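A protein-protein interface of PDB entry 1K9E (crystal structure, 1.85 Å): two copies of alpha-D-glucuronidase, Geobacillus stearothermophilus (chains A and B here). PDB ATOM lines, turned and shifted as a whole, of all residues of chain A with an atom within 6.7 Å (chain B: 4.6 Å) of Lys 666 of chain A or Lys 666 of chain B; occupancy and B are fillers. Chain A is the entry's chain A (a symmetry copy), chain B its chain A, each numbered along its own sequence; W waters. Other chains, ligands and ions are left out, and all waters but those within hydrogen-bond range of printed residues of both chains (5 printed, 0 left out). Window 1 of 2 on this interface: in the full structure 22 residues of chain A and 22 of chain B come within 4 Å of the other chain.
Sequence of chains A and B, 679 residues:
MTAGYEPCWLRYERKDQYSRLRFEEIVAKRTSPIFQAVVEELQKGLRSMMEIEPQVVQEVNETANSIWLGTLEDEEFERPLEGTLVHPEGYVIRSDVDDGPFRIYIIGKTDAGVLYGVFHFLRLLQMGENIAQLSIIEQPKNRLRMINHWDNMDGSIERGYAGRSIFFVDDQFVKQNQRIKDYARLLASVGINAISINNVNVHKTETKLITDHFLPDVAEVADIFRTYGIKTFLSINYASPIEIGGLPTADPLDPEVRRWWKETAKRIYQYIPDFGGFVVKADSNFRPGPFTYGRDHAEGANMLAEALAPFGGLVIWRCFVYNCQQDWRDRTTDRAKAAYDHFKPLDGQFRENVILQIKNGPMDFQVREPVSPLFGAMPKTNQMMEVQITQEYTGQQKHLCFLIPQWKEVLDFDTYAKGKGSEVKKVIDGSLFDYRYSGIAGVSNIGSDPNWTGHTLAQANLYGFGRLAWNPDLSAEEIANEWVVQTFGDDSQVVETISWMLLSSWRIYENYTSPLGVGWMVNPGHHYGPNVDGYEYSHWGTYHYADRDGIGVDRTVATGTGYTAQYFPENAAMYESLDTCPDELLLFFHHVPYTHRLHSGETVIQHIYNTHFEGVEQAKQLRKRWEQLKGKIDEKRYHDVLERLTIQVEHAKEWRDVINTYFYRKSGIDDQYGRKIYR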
ATOM      1  N   ASP A 533      27.051   0.708 -12.468  1.00  0.00           N
ATOM      2  CA  ASP A 533      27.311   1.552 -11.295  1.00  0.00           C
ATOM      3  C   ASP A 533      26.985   0.859  -9.974  1.00  0.00           C
ATOM      4  O   ASP A 533      26.944   1.503  -8.928  1.00  0.00           O
ATOM      5  CB  ASP A 533      26.519   2.862 -11.387  1.00  0.00           C
ATOM      6  CG  ASP A 533      27.224   3.915 -12.238  1.00  0.00           C
ATOM      7  OD1 ASP A 533      28.198   3.570 -12.939  1.00  0.00           O
ATOM      8  OD2 ASP A 533      26.797   5.088 -12.202  1.00  0.00           O
ATOM      9  N   GLU A 536      29.729   1.600  -7.731  1.00  0.00           N
ATOM     10  CA  GLU A 536      30.473   2.792  -8.124  1.00  0.00           C
ATOM     11  C   GLU A 536      30.554   3.914  -7.087  1.00  0.00           C
ATOM     12  O   GLU A 536      31.507   4.696  -7.093  1.00  0.00           O
ATOM     13  CB  GLU A 536      29.916   3.323  -9.446  1.00  0.00           C
ATOM     14  CG  GLU A 536      30.723   4.443 -10.079  1.00  0.00           C
ATOM     15  CD  GLU A 536      32.160   4.057 -10.401  1.00  0.00           C
ATOM     16  OE1 GLU A 536      32.501   2.856 -10.362  1.00  0.00           O
ATOM     17  OE2 GLU A 536      32.954   4.972 -10.712  1.00  0.00           O
ATOM     18  N   TYR A 537      29.556   4.012  -6.214  1.00  0.00           N
ATOM     19  CA  TYR A 537      29.578   5.028  -5.171  1.00  0.00           C
ATOM     20  C   TYR A 537      29.481   4.374  -3.802  1.00  0.00           C
ATOM     21  O   TYR A 537      28.962   4.963  -2.852  1.00  0.00           O
ATOM     22  CB  TYR A 537      28.444   6.036  -5.356  1.00  0.00           C
ATOM     23  CG  TYR A 537      28.525   6.762  -6.677  1.00  0.00           C
ATOM     24  CD1 TYR A 537      27.968   6.213  -7.831  1.00  0.00           C
ATOM     25  CD2 TYR A 537      29.203   7.976  -6.784  1.00  0.00           C
ATOM     26  CE1 TYR A 537      28.083   6.852  -9.061  1.00  0.00           C
ATOM     27  CE2 TYR A 537      29.324   8.625  -8.009  1.00  0.00           C
ATOM     28  CZ  TYR A 537      28.764   8.059  -9.142  1.00  0.00           C
ATOM     29  OH  TYR A 537      28.897   8.694 -10.358  1.00  0.00           O
ATOM     30  N   HIS A 544      35.214   2.320 -11.296  1.00  0.00           N
ATOM     31  CA  HIS A 544      35.702   2.368 -12.665  1.00  0.00           C
ATOM     32  C   HIS A 544      35.853   3.824 -13.123  1.00  0.00           C
ATOM     33  O   HIS A 544      36.519   4.106 -14.121  1.00  0.00           O
ATOM     34  CB  HIS A 544      34.772   1.587 -13.608  1.00  0.00           C
ATOM     35  CG  HIS A 544      33.328   1.960 -13.497  1.00  0.00           C
ATOM     36  ND1 HIS A 544      32.866   3.236 -13.736  1.00  0.00           N
ATOM     37  CD2 HIS A 544      32.238   1.221 -13.171  1.00  0.00           C
ATOM     38  CE1 HIS A 544      31.557   3.269 -13.560  1.00  0.00           C
ATOM     39  NE2 HIS A 544      31.152   2.059 -13.215  1.00  0.00           N
ATOM     40  N   TYR A 545      35.231   4.742 -12.383  1.00  0.00           N
ATOM     41  CA  TYR A 545      35.310   6.178 -12.676  1.00  0.00           C
ATOM     42  C   TYR A 545      34.857   6.584 -14.072  1.00  0.00           C
ATOM     43  O   TYR A 545      35.330   7.585 -14.618  1.00  0.00           O
ATOM     44  CB  TYR A 545      36.738   6.686 -12.470  1.00  0.00           C
ATOM     45  CG  TYR A 545      37.286   6.452 -11.084  1.00  0.00           C
ATOM     46  CD1 TYR A 545      36.743   7.099  -9.976  1.00  0.00           C
ATOM     47  CD2 TYR A 545      38.342   5.571 -10.879  1.00  0.00           C
ATOM     48  CE1 TYR A 545      37.244   6.868  -8.689  1.00  0.00           C
ATOM     49  CE2 TYR A 545      38.845   5.331  -9.608  1.00  0.00           C
ATOM     50  CZ  TYR A 545      38.297   5.979  -8.520  1.00  0.00           C
ATOM     51  OH  TYR A 545      38.801   5.719  -7.267  1.00  0.00           O
ATOM     52  N   ALA A 546      33.944   5.828 -14.659  1.00  0.00           N
ATOM     53  CA  ALA A 546      33.482   6.187 -15.988  1.00  0.00           C
ATOM     54  C   ALA A 546      32.716   7.510 -15.969  1.00  0.00           C
ATOM     55  O   ALA A 546      31.936   7.780 -15.057  1.00  0.00           O
ATOM     56  CB  ALA A 546      32.600   5.088 -16.553  1.00  0.00           C
ATOM     57  N   ASP A 547      32.976   8.350 -16.963  1.00  0.00           N
ATOM     58  CA  ASP A 547      32.260   9.605 -17.085  1.00  0.00           C
ATOM     59  C   ASP A 547      31.999   9.815 -18.570  1.00  0.00           C
ATOM     60  O   ASP A 547      32.242   8.912 -19.368  1.00  0.00           O
ATOM     61  CB  ASP A 547      33.025  10.790 -16.458  1.00  0.00           C
ATOM     62  CG  ASP A 547      34.431  10.960 -17.002  1.00  0.00           C
ATOM     63  OD1 ASP A 547      34.661  10.663 -18.187  1.00  0.00           O
ATOM     64  OD2 ASP A 547      35.301  11.425 -16.231  1.00  0.00           O
ATOM     65  N   ARG A 548      31.508  10.985 -18.949  1.00  0.00           N
ATOM     66  CA  ARG A 548      31.188  11.218 -20.353  1.00  0.00           C
ATOM     67  C   ARG A 548      32.383  11.221 -21.305  1.00  0.00           C
ATOM     68  O   ARG A 548      32.200  11.120 -22.518  1.00  0.00           O
ATOM     69  CB  ARG A 548      30.391  12.525 -20.494  1.00  0.00           C
ATOM     70  CG  ARG A 548      31.229  13.801 -20.466  1.00  0.00           C
ATOM     71  CD  ARG A 548      30.374  15.010 -20.084  1.00  0.00           C
ATOM     72  NE  ARG A 548      29.125  15.115 -20.842  1.00  0.00           N
ATOM     73  CZ  ARG A 548      29.002  15.706 -22.026  1.00  0.00           C
ATOM     74  NH1 ARG A 548      30.055  16.257 -22.616  1.00  0.00           N
ATOM     75  NH2 ARG A 548      27.817  15.762 -22.616  1.00  0.00           N
ATOM     76  N   ASP A 549      33.599  11.314 -20.767  1.00  0.00           N
ATOM     77  CA  ASP A 549      34.791  11.348 -21.614  1.00  0.00           C
ATOM     78  C   ASP A 549      35.642  10.082 -21.625  1.00  0.00           C
ATOM     79  O   ASP A 549      36.261   9.754 -22.636  1.00  0.00           O
ATOM     80  CB  ASP A 549      35.697  12.519 -21.212  1.00  0.00           C
ATOM     81  CG  ASP A 549      34.993  13.859 -21.292  1.00  0.00           C
ATOM     82  OD1 ASP A 549      34.381  14.148 -22.339  1.00  0.00           O
ATOM     83  OD2 ASP A 549      35.060  14.621 -20.308  1.00  0.00           O
ATOM     84  N   GLY A 550      35.699   9.381 -20.499  1.00  0.00           N
ATOM     85  CA  GLY A 550      36.527   8.193 -20.457  1.00  0.00           C
ATOM     86  C   GLY A 550      36.264   7.299 -19.267  1.00  0.00           C
ATOM     87  O   GLY A 550      35.270   7.468 -18.558  1.00  0.00           O
ATOM     88  N   TYR A 594      37.536   7.492 -24.022  1.00  0.00           N
ATOM     89  CA  TYR A 594      36.870   6.422 -24.761  1.00  0.00           C
ATOM     90  C   TYR A 594      37.485   6.247 -26.145  1.00  0.00           C
ATOM     91  O   TYR A 594      37.440   5.166 -26.727  1.00  0.00           O
ATOM     92  CB  TYR A 594      35.374   6.724 -24.908  1.00  0.00           C
ATOM     93  CG  TYR A 594      34.594   6.596 -23.621  1.00  0.00           C
ATOM     94  CD1 TYR A 594      34.567   5.389 -22.916  1.00  0.00           C
ATOM     95  CD2 TYR A 594      33.895   7.681 -23.099  1.00  0.00           C
ATOM     96  CE1 TYR A 594      33.867   5.266 -21.716  1.00  0.00           C
ATOM     97  CE2 TYR A 594      33.188   7.572 -21.902  1.00  0.00           C
ATOM     98  CZ  TYR A 594      33.182   6.362 -21.216  1.00  0.00           C
ATOM     99  OH  TYR A 594      32.519   6.257 -20.019  1.00  0.00           O
ATOM    100  N   THR A 661      24.308  -0.023 -23.531  1.00  0.00           N
ATOM    101  CA  THR A 661      23.465   1.151 -23.332  1.00  0.00           C
ATOM    102  C   THR A 661      24.091   2.134 -22.353  1.00  0.00           C
ATOM    103  O   THR A 661      24.100   3.339 -22.601  1.00  0.00           O
ATOM    104  CB  THR A 661      22.063   0.757 -22.839  1.00  0.00           C
ATOM    105  OG1 THR A 661      21.379   0.061 -23.889  1.00  0.00           O
ATOM    106  CG2 THR A 661      21.253   1.998 -22.442  1.00  0.00           C
ATOM    107  N   TYR A 662      24.621   1.625 -21.246  1.00  0.00           N
ATOM    108  CA  TYR A 662      25.246   2.493 -20.256  1.00  0.00           C
ATOM    109  C   TYR A 662      26.350   3.320 -20.894  1.00  0.00           C
ATOM    110  O   TYR A 662      26.432   4.531 -20.685  1.00  0.00           O
ATOM    111  CB  TYR A 662      25.834   1.664 -19.107  1.00  0.00           C
ATOM    112  CG  TYR A 662      26.582   2.474 -18.057  1.00  0.00           C
ATOM    113  CD1 TYR A 662      27.869   2.965 -18.302  1.00  0.00           C
ATOM    114  CD2 TYR A 662      26.004   2.743 -16.815  1.00  0.00           C
ATOM    115  CE1 TYR A 662      28.562   3.703 -17.333  1.00  0.00           C
ATOM    116  CE2 TYR A 662      26.691   3.484 -15.834  1.00  0.00           C
ATOM    117  CZ  TYR A 662      27.966   3.957 -16.103  1.00  0.00           C
ATOM    118  OH  TYR A 662      28.648   4.676 -15.138  1.00  0.00           O
ATOM    119  N   PHE A 663      27.209   2.675 -21.673  1.00  0.00           N
ATOM    120  CA  PHE A 663      28.308   3.414 -22.278  1.00  0.00           C
ATOM    121  C   PHE A 663      27.906   4.274 -23.453  1.00  0.00           C
ATOM    122  O   PHE A 663      28.573   5.261 -23.756  1.00  0.00           O
ATOM    123  CB  PHE A 663      29.464   2.467 -22.604  1.00  0.00           C
ATOM    124  CG  PHE A 663      30.225   2.062 -21.380  1.00  0.00           C
ATOM    125  CD1 PHE A 663      31.053   2.979 -20.732  1.00  0.00           C
ATOM    126  CD2 PHE A 663      30.010   0.826 -20.793  1.00  0.00           C
ATOM    127  CE1 PHE A 663      31.646   2.672 -19.512  1.00  0.00           C
ATOM    128  CE2 PHE A 663      30.600   0.504 -19.567  1.00  0.00           C
ATOM    129  CZ  PHE A 663      31.417   1.432 -18.927  1.00  0.00           C
ATOM    130  N   TYR A 664      26.804   3.930 -24.105  1.00  0.00           N
ATOM    131  CA  TYR A 664      26.346   4.787 -25.187  1.00  0.00           C
ATOM    132  C   TYR A 664      25.757   6.036 -24.518  1.00  0.00           C
ATOM    133  O   TYR A 664      26.024   7.167 -24.929  1.00  0.00           O
ATOM    134  CB  TYR A 664      25.260   4.116 -26.023  1.00  0.00           C
ATOM    135  CG  TYR A 664      24.640   5.087 -27.001  1.00  0.00           C
ATOM    136  CD1 TYR A 664      25.360   5.548 -28.102  1.00  0.00           C
ATOM    137  CD2 TYR A 664      23.369   5.614 -26.776  1.00  0.00           C
ATOM    138  CE1 TYR A 664      24.831   6.517 -28.953  1.00  0.00           C
ATOM    139  CE2 TYR A 664      22.832   6.582 -27.617  1.00  0.00           C
ATOM    140  CZ  TYR A 664      23.569   7.032 -28.701  1.00  0.00           C
ATOM    141  OH  TYR A 664      23.051   8.014 -29.513  1.00  0.00           O
ATOM    142  N   ARG A 665      24.957   5.830 -23.475  1.00  0.00           N
ATOM    143  CA  ARG A 665      24.351   6.961 -22.780  1.00  0.00           C
ATOM    144  C   ARG A 665      25.389   7.898 -22.178  1.00  0.00           C
ATOM    145  O   ARG A 665      25.147   9.091 -22.051  1.00  0.00           O
ATOM    146  CB  ARG A 665      23.402   6.481 -21.681  1.00  0.00           C
ATOM    147  CG  ARG A 665      22.064   5.980 -22.211  1.00  0.00           C
ATOM    148  CD  ARG A 665      21.179   5.474 -21.087  1.00  0.00           C
ATOM    149  NE  ARG A 665      19.934   4.912 -21.602  1.00  0.00           N
ATOM    150  CZ  ARG A 665      19.092   4.187 -20.877  1.00  0.00           C
ATOM    151  NH1 ARG A 665      19.364   3.937 -19.605  1.00  0.00           N
ATOM    152  NH2 ARG A 665      17.985   3.702 -21.424  1.00  0.00           N
ATOM    153  N   LYS A 666      26.552   7.368 -21.823  1.00  0.00           N
ATOM    154  CA  LYS A 666      27.584   8.202 -21.230  1.00  0.00           C
ATOM    155  C   LYS A 666      28.593   8.757 -22.247  1.00  0.00           C
ATOM    156  O   LYS A 666      28.965   9.929 -22.182  1.00  0.00           O
ATOM    157  CB  LYS A 666      28.296   7.409 -20.122  1.00  0.00           C
ATOM    158  CG  LYS A 666      29.264   8.222 -19.292  1.00  0.00           C
ATOM    159  CD  LYS A 666      29.593   7.559 -17.945  1.00  0.00           C
ATOM    160  CE  LYS A 666      28.543   7.876 -16.892  1.00  0.00           C
ATOM    161  NZ  LYS A 666      28.999   7.551 -15.499  1.00  0.00           N
ATOM    162  N   SER A 667      29.017   7.930 -23.198  1.00  0.00           N
ATOM    163  CA  SER A 667      30.000   8.362 -24.190  1.00  0.00           C
ATOM    164  C   SER A 667      29.373   9.090 -25.372  1.00  0.00           C
ATOM    165  O   SER A 667      29.999   9.966 -25.969  1.00  0.00           O
ATOM    166  CB  SER A 667      30.785   7.160 -24.722  1.00  0.00           C
ATOM    167  OG  SER A 667      30.023   6.435 -25.678  1.00  0.00           O
ATOM    168  N   GLY A 668      28.146   8.712 -25.715  1.00  0.00           N
ATOM    169  CA  GLY A 668      27.471   9.332 -26.843  1.00  0.00           C
ATOM    170  C   GLY A 668      28.023   8.853 -28.173  1.00  0.00           C
ATOM    171  O   GLY A 668      27.648   9.361 -29.232  1.00  0.00           O
ATOM    172  N   ILE A 669      28.917   7.870 -28.128  1.00  0.00           N
ATOM    173  CA  ILE A 669      29.524   7.335 -29.345  1.00  0.00           C
ATOM    174  C   ILE A 669      28.795   6.074 -29.803  1.00  0.00           C
ATOM    175  O   ILE A 669      28.624   5.133 -29.035  1.00  0.00           O
ATOM    176  CB  ILE A 669      31.022   7.035 -29.105  1.00  0.00           C
ATOM    177  CG1 ILE A 669      31.744   8.341 -28.760  1.00  0.00           C
ATOM    178  CG2 ILE A 669      31.646   6.399 -30.345  1.00  0.00           C
ATOM    179  CD1 ILE A 669      33.112   8.154 -28.125  1.00  0.00           C
ATOM    180  N   ALA B 546      18.641   9.029 -17.603  1.00  0.00           N
ATOM    181  CA  ALA B 546      19.667  10.052 -17.702  1.00  0.00           C
ATOM    182  C   ALA B 546      20.794   9.616 -18.637  1.00  0.00           C
ATOM    183  O   ALA B 546      21.212   8.460 -18.634  1.00  0.00           O
ATOM    184  CB  ALA B 546      20.229  10.366 -16.327  1.00  0.00           C
ATOM    185  N   ASP B 547      21.255  10.543 -19.468  1.00  0.00           N
ATOM    186  CA  ASP B 547      22.369  10.264 -20.354  1.00  0.00           C
ATOM    187  C   ASP B 547      23.228  11.520 -20.383  1.00  0.00           C
ATOM    188  O   ASP B 547      22.993  12.441 -19.604  1.00  0.00           O
ATOM    189  CB  ASP B 547      21.914   9.839 -21.766  1.00  0.00           C
ATOM    190  CG  ASP B 547      20.985  10.838 -22.430  1.00  0.00           C
ATOM    191  OD1 ASP B 547      21.128  12.050 -22.189  1.00  0.00           O
ATOM    192  OD2 ASP B 547      20.124  10.395 -23.223  1.00  0.00           O
ATOM    193  N   ARG B 548      24.216  11.569 -21.263  1.00  0.00           N
ATOM    194  CA  ARG B 548      25.103  12.727 -21.295  1.00  0.00           C
ATOM    195  C   ARG B 548      24.446  14.043 -21.706  1.00  0.00           C
ATOM    196  O   ARG B 548      25.023  15.110 -21.490  1.00  0.00           O
ATOM    197  CB  ARG B 548      26.313  12.430 -22.197  1.00  0.00           C
ATOM    198  CG  ARG B 548      26.054  12.578 -23.695  1.00  0.00           C
ATOM    199  CD  ARG B 548      27.080  11.785 -24.507  1.00  0.00           C
ATOM    200  NE  ARG B 548      28.467  12.019 -24.100  1.00  0.00           N
ATOM    201  CZ  ARG B 548      29.235  13.008 -24.547  1.00  0.00           C
ATOM    202  NH1 ARG B 548      28.762  13.881 -25.428  1.00  0.00           N
ATOM    203  NH2 ARG B 548      30.486  13.115 -24.125  1.00  0.00           N
ATOM    204  N   TYR B 594      19.724  18.829 -20.079  1.00  0.00           N
ATOM    205  CA  TYR B 594      20.178  19.380 -18.805  1.00  0.00           C
ATOM    206  C   TYR B 594      20.114  20.903 -18.814  1.00  0.00           C
ATOM    207  O   TYR B 594      19.977  21.538 -17.770  1.00  0.00           O
ATOM    208  CB  TYR B 594      21.618  18.939 -18.514  1.00  0.00           C
ATOM    209  CG  TYR B 594      21.749  17.476 -18.158  1.00  0.00           C
ATOM    210  CD1 TYR B 594      21.065  16.940 -17.063  1.00  0.00           C
ATOM    211  CD2 TYR B 594      22.543  16.625 -18.922  1.00  0.00           C
ATOM    212  CE1 TYR B 594      21.163  15.588 -16.739  1.00  0.00           C
ATOM    213  CE2 TYR B 594      22.654  15.271 -18.607  1.00  0.00           C
ATOM    214  CZ  TYR B 594      21.957  14.760 -17.517  1.00  0.00           C
ATOM    215  OH  TYR B 594      22.032  13.421 -17.223  1.00  0.00           O
ATOM    216  N   TYR B 662      27.524  12.154  -9.904  1.00  0.00           N
ATOM    217  CA  TYR B 662      26.936  11.376 -10.987  1.00  0.00           C
ATOM    218  C   TYR B 662      26.539  12.283 -12.140  1.00  0.00           C
ATOM    219  O   TYR B 662      26.833  11.994 -13.300  1.00  0.00           O
ATOM    220  CB  TYR B 662      25.699  10.614 -10.493  1.00  0.00           C
ATOM    221  CG  TYR B 662      24.962   9.832 -11.572  1.00  0.00           C
ATOM    222  CD1 TYR B 662      24.139  10.478 -12.500  1.00  0.00           C
ATOM    223  CD2 TYR B 662      25.084   8.444 -11.658  1.00  0.00           C
ATOM    224  CE1 TYR B 662      23.453   9.757 -13.488  1.00  0.00           C
ATOM    225  CE2 TYR B 662      24.400   7.711 -12.647  1.00  0.00           C
ATOM    226  CZ  TYR B 662      23.589   8.376 -13.553  1.00  0.00           C
ATOM    227  OH  TYR B 662      22.907   7.657 -14.519  1.00  0.00           O
ATOM    228  N   PHE B 663      25.866  13.386 -11.832  1.00  0.00           N
ATOM    229  CA  PHE B 663      25.429  14.270 -12.903  1.00  0.00           C
ATOM    230  C   PHE B 663      26.529  15.120 -13.495  1.00  0.00           C
ATOM    231  O   PHE B 663      26.436  15.540 -14.645  1.00  0.00           O
ATOM    232  CB  PHE B 663      24.223  15.092 -12.449  1.00  0.00           C
ATOM    233  CG  PHE B 663      22.966  14.280 -12.416  1.00  0.00           C
ATOM    234  CD1 PHE B 663      22.351  13.888 -13.606  1.00  0.00           C
ATOM    235  CD2 PHE B 663      22.475  13.787 -11.218  1.00  0.00           C
ATOM    236  CE1 PHE B 663      21.274  13.008 -13.600  1.00  0.00           C
ATOM    237  CE2 PHE B 663      21.393  12.903 -11.198  1.00  0.00           C
ATOM    238  CZ  PHE B 663      20.795  12.512 -12.393  1.00  0.00           C
ATOM    239  N   TYR B 664      27.587  15.357 -12.732  1.00  0.00           N
ATOM    240  CA  TYR B 664      28.698  16.100 -13.303  1.00  0.00           C
ATOM    241  C   TYR B 664      29.403  15.136 -14.267  1.00  0.00           C
ATOM    242  O   TYR B 664      29.744  15.496 -15.394  1.00  0.00           O
ATOM    243  CB  TYR B 664      29.693  16.547 -12.236  1.00  0.00           C
ATOM    244  CG  TYR B 664      30.943  17.123 -12.856  1.00  0.00           C
ATOM    245  CD1 TYR B 664      30.916  18.357 -13.505  1.00  0.00           C
ATOM    246  CD2 TYR B 664      32.133  16.396 -12.874  1.00  0.00           C
ATOM    247  CE1 TYR B 664      32.040  18.850 -14.163  1.00  0.00           C
ATOM    248  CE2 TYR B 664      33.261  16.877 -13.529  1.00  0.00           C
ATOM    249  CZ  TYR B 664      33.208  18.102 -14.175  1.00  0.00           C
ATOM    250  OH  TYR B 664      34.313  18.562 -14.851  1.00  0.00           O
ATOM    251  N   ARG B 665      29.615  13.900 -13.821  1.00  0.00           N
ATOM    252  CA  ARG B 665      30.282  12.918 -14.669  1.00  0.00           C
ATOM    253  C   ARG B 665      29.514  12.643 -15.955  1.00  0.00           C
ATOM    254  O   ARG B 665      30.107  12.312 -16.972  1.00  0.00           O
ATOM    255  CB  ARG B 665      30.500  11.605 -13.916  1.00  0.00           C
ATOM    256  CG  ARG B 665      31.655  11.659 -12.925  1.00  0.00           C
ATOM    257  CD  ARG B 665      31.800  10.348 -12.173  1.00  0.00           C
ATOM    258  NE  ARG B 665      32.847  10.428 -11.160  1.00  0.00           N
ATOM    259  CZ  ARG B 665      33.026   9.526 -10.204  1.00  0.00           C
ATOM    260  NH1 ARG B 665      32.223   8.475 -10.133  1.00  0.00           N
ATOM    261  NH2 ARG B 665      33.997   9.678  -9.314  1.00  0.00           N
ATOM    262  N   LYS B 666      28.197  12.795 -15.918  1.00  0.00           N
ATOM    263  CA  LYS B 666      27.399  12.536 -17.106  1.00  0.00           C
ATOM    264  C   LYS B 666      27.127  13.787 -17.955  1.00  0.00           C
ATOM    265  O   LYS B 666      27.214  13.741 -19.182  1.00  0.00           O
ATOM    266  CB  LYS B 666      26.086  11.854 -16.691  1.00  0.00           C
ATOM    267  CG  LYS B 666      25.245  11.355 -17.845  1.00  0.00           C
ATOM    268  CD  LYS B 666      24.215  10.298 -17.416  1.00  0.00           C
ATOM    269  CE  LYS B 666      24.828   8.908 -17.360  1.00  0.00           C
ATOM    270  NZ  LYS B 666      23.796   7.820 -17.294  1.00  0.00           N
ATOM    271  N   SER B 667      26.823  14.909 -17.307  1.00  0.00           N
ATOM    272  CA  SER B 667      26.519  16.140 -18.033  1.00  0.00           C
ATOM    273  C   SER B 667      27.764  16.928 -18.417  1.00  0.00           C
ATOM    274  O   SER B 667      27.777  17.618 -19.437  1.00  0.00           O
ATOM    275  CB  SER B 667      25.612  17.044 -17.194  1.00  0.00           C
ATOM    276  OG  SER B 667      26.356  17.726 -16.193  1.00  0.00           O
ATOM    277  N   GLY B 668      28.800  16.837 -17.589  1.00  0.00           N
ATOM    278  CA  GLY B 668      30.026  17.569 -17.858  1.00  0.00           C
ATOM    279  C   GLY B 668      29.882  19.051 -17.563  1.00  0.00           C
ATOM    280  O   GLY B 668      30.787  19.841 -17.844  1.00  0.00           O
HETATM  281  O   HOH W   1      20.216   6.103 -17.517  1.00  0.00           O
HETATM  282  O   HOH W   2      25.549   5.785 -18.315  1.00  0.00           O
HETATM  283  O   HOH W   3      33.200   6.490  -8.242  1.00  0.00           O
HETATM  284  O   HOH W   4      27.148   9.348 -14.233  1.00  0.00           O
HETATM  285  O   HOH W   5      31.502   6.629 -12.551  1.00  0.00           O
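Arg 548 of chain B touches its own counterpart, Arg 548 of chain A. Arg 548 of chain A touches Lys 666 of chain B, and with the chains exchanged Lys 666 of chain A touches Arg 548 of chain B. Arg 548 of chain A touches Ser 667 of chain B, and with the chains exchanged Ser 667 of chain A touches Arg 548 of chain B.
Printed residues of chain B that touch a printed residue of chain A: Ala 546, Asp 547, Arg 548, Tyr 662, Arg 665, Lys 666, Ser 667 and Gly 668. Hydrophobic or aromatic side chains of chain B that line the printed part of chain A: Tyr 662.
Printed residues of chain B within 4 Å of Tyr 537 of chain A: Tyr 662 and Arg 665. Of the printed residues of chain B, Arg 548 of chain A touches Arg 548 (3.1 Å), Arg 665 (2.8 Å), Lys 666 (2.9 Å), Ser 667 (3.2 Å) and Gly 668 (3.4 Å). Thr 661 of chain A touches none of the printed residues of chain B. Lys 666 of chain A touches just these residues of chain B: Arg 548 (2.9 Å) and Lys 666 (3.9 Å). Lys 666 of chain B touches just these residues of chain A: Arg 548 and Lys 666. The nearest printed residue of chain B that does not touch Lys 666 of chain A is Arg 665 of chain B (4.6 Å). The nearest printed residue of chain B that does not touch Tyr 545 of chain A is Lys 666 of chain B (8.9 Å).
The guanidinium group of Arg 548 of chain A is in hydrogen-bond range of the backbone carbonyl oxygen of Arg 548 of chain B (3.1 Å). N of Arg 548 of chain B lies within hydrogen-bond range of O of Arg 665 of chain A, 2.8 Å away. The backbone carbonyl oxygen (O) of Lys 666 of chain A sits at hydrogen-bond distance from the guanidinium group (NE) of Arg 548 of chain B (2.9 Å). The backbone carbonyl oxygen (O) of Ser 667 of chain A lies within hydrogen-bond range of the guanidinium group (NE) of Arg 548 of chain B (3.2 Å). NH1 of Arg 665 of chain B lies within salt-bridge range of OE2 of Glu 536 of chain A (3.6 Å). The guanidinium group (NH1) of Arg 665 of chain B sits at hydrogen-bond distance from the side-chain hydroxyl (OH) of Tyr 537 of chain A. O of Arg 665 of chain B sits at hydrogen-bond distance from N of Arg 548 of chain A (2.8 Å). The backbone carbonyl oxygen (O) of Lys 666 of chain B sits at hydrogen-bond distance from the guanidinium group (NE) of Arg 548 of chain A (2.9 Å). O of Ser 667 of chain B is in hydrogen-bond range of NE of Arg 548 of chain A, at 3.2 Å.
Among the printed residues, pairs that only touch across the chains: Arg 665 of chain A with Asp 547 of chain B (3.3 Å), Asp 547 of chain A with Arg 665 of chain B (3.3 Å), Tyr 537 of chain A with Tyr 662 of chain B (3.4 Å), Arg 548 of chain A with Gly 668 of chain B (3.4 Å), Gly 668 of chain A with Arg 548 of chain B (3.4 Å), Asp 533 of chain A with Tyr 662 of chain B (3.6 Å), Tyr 545 of chain A with Arg 665 of chain B (3.8 Å), Ala 546 of chain A with Arg 665 of chain B (3.9 Å), Arg 665 of chain A with Ala 546 of chain B (3.9 Å) and Lys 666 of chain A with Lys 666 of chain B (3.9 Å).
Water W1 bridges the backbone carbonyl oxygen of Ala 546 of chain B (2.8 Å) and the guanidinium group of Arg 665 of chain A (3.1 Å). Water W2 lies within hydrogen-bond range of the backbone carbonyl oxygen (O) of Tyr 662 of chain A and the side-chain amino group (NZ) of Lys 666 of chain B.
NE2 of His 544 of chain A is in hydrogen-bond range of OD1 of Asp 533 of chain A (3.3 Å). The backbone NH (N) of Ala 546 of chain A sits at hydrogen-bond distance from a ring nitrogen (ND1) of His 544 of chain A (3.0 Å).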
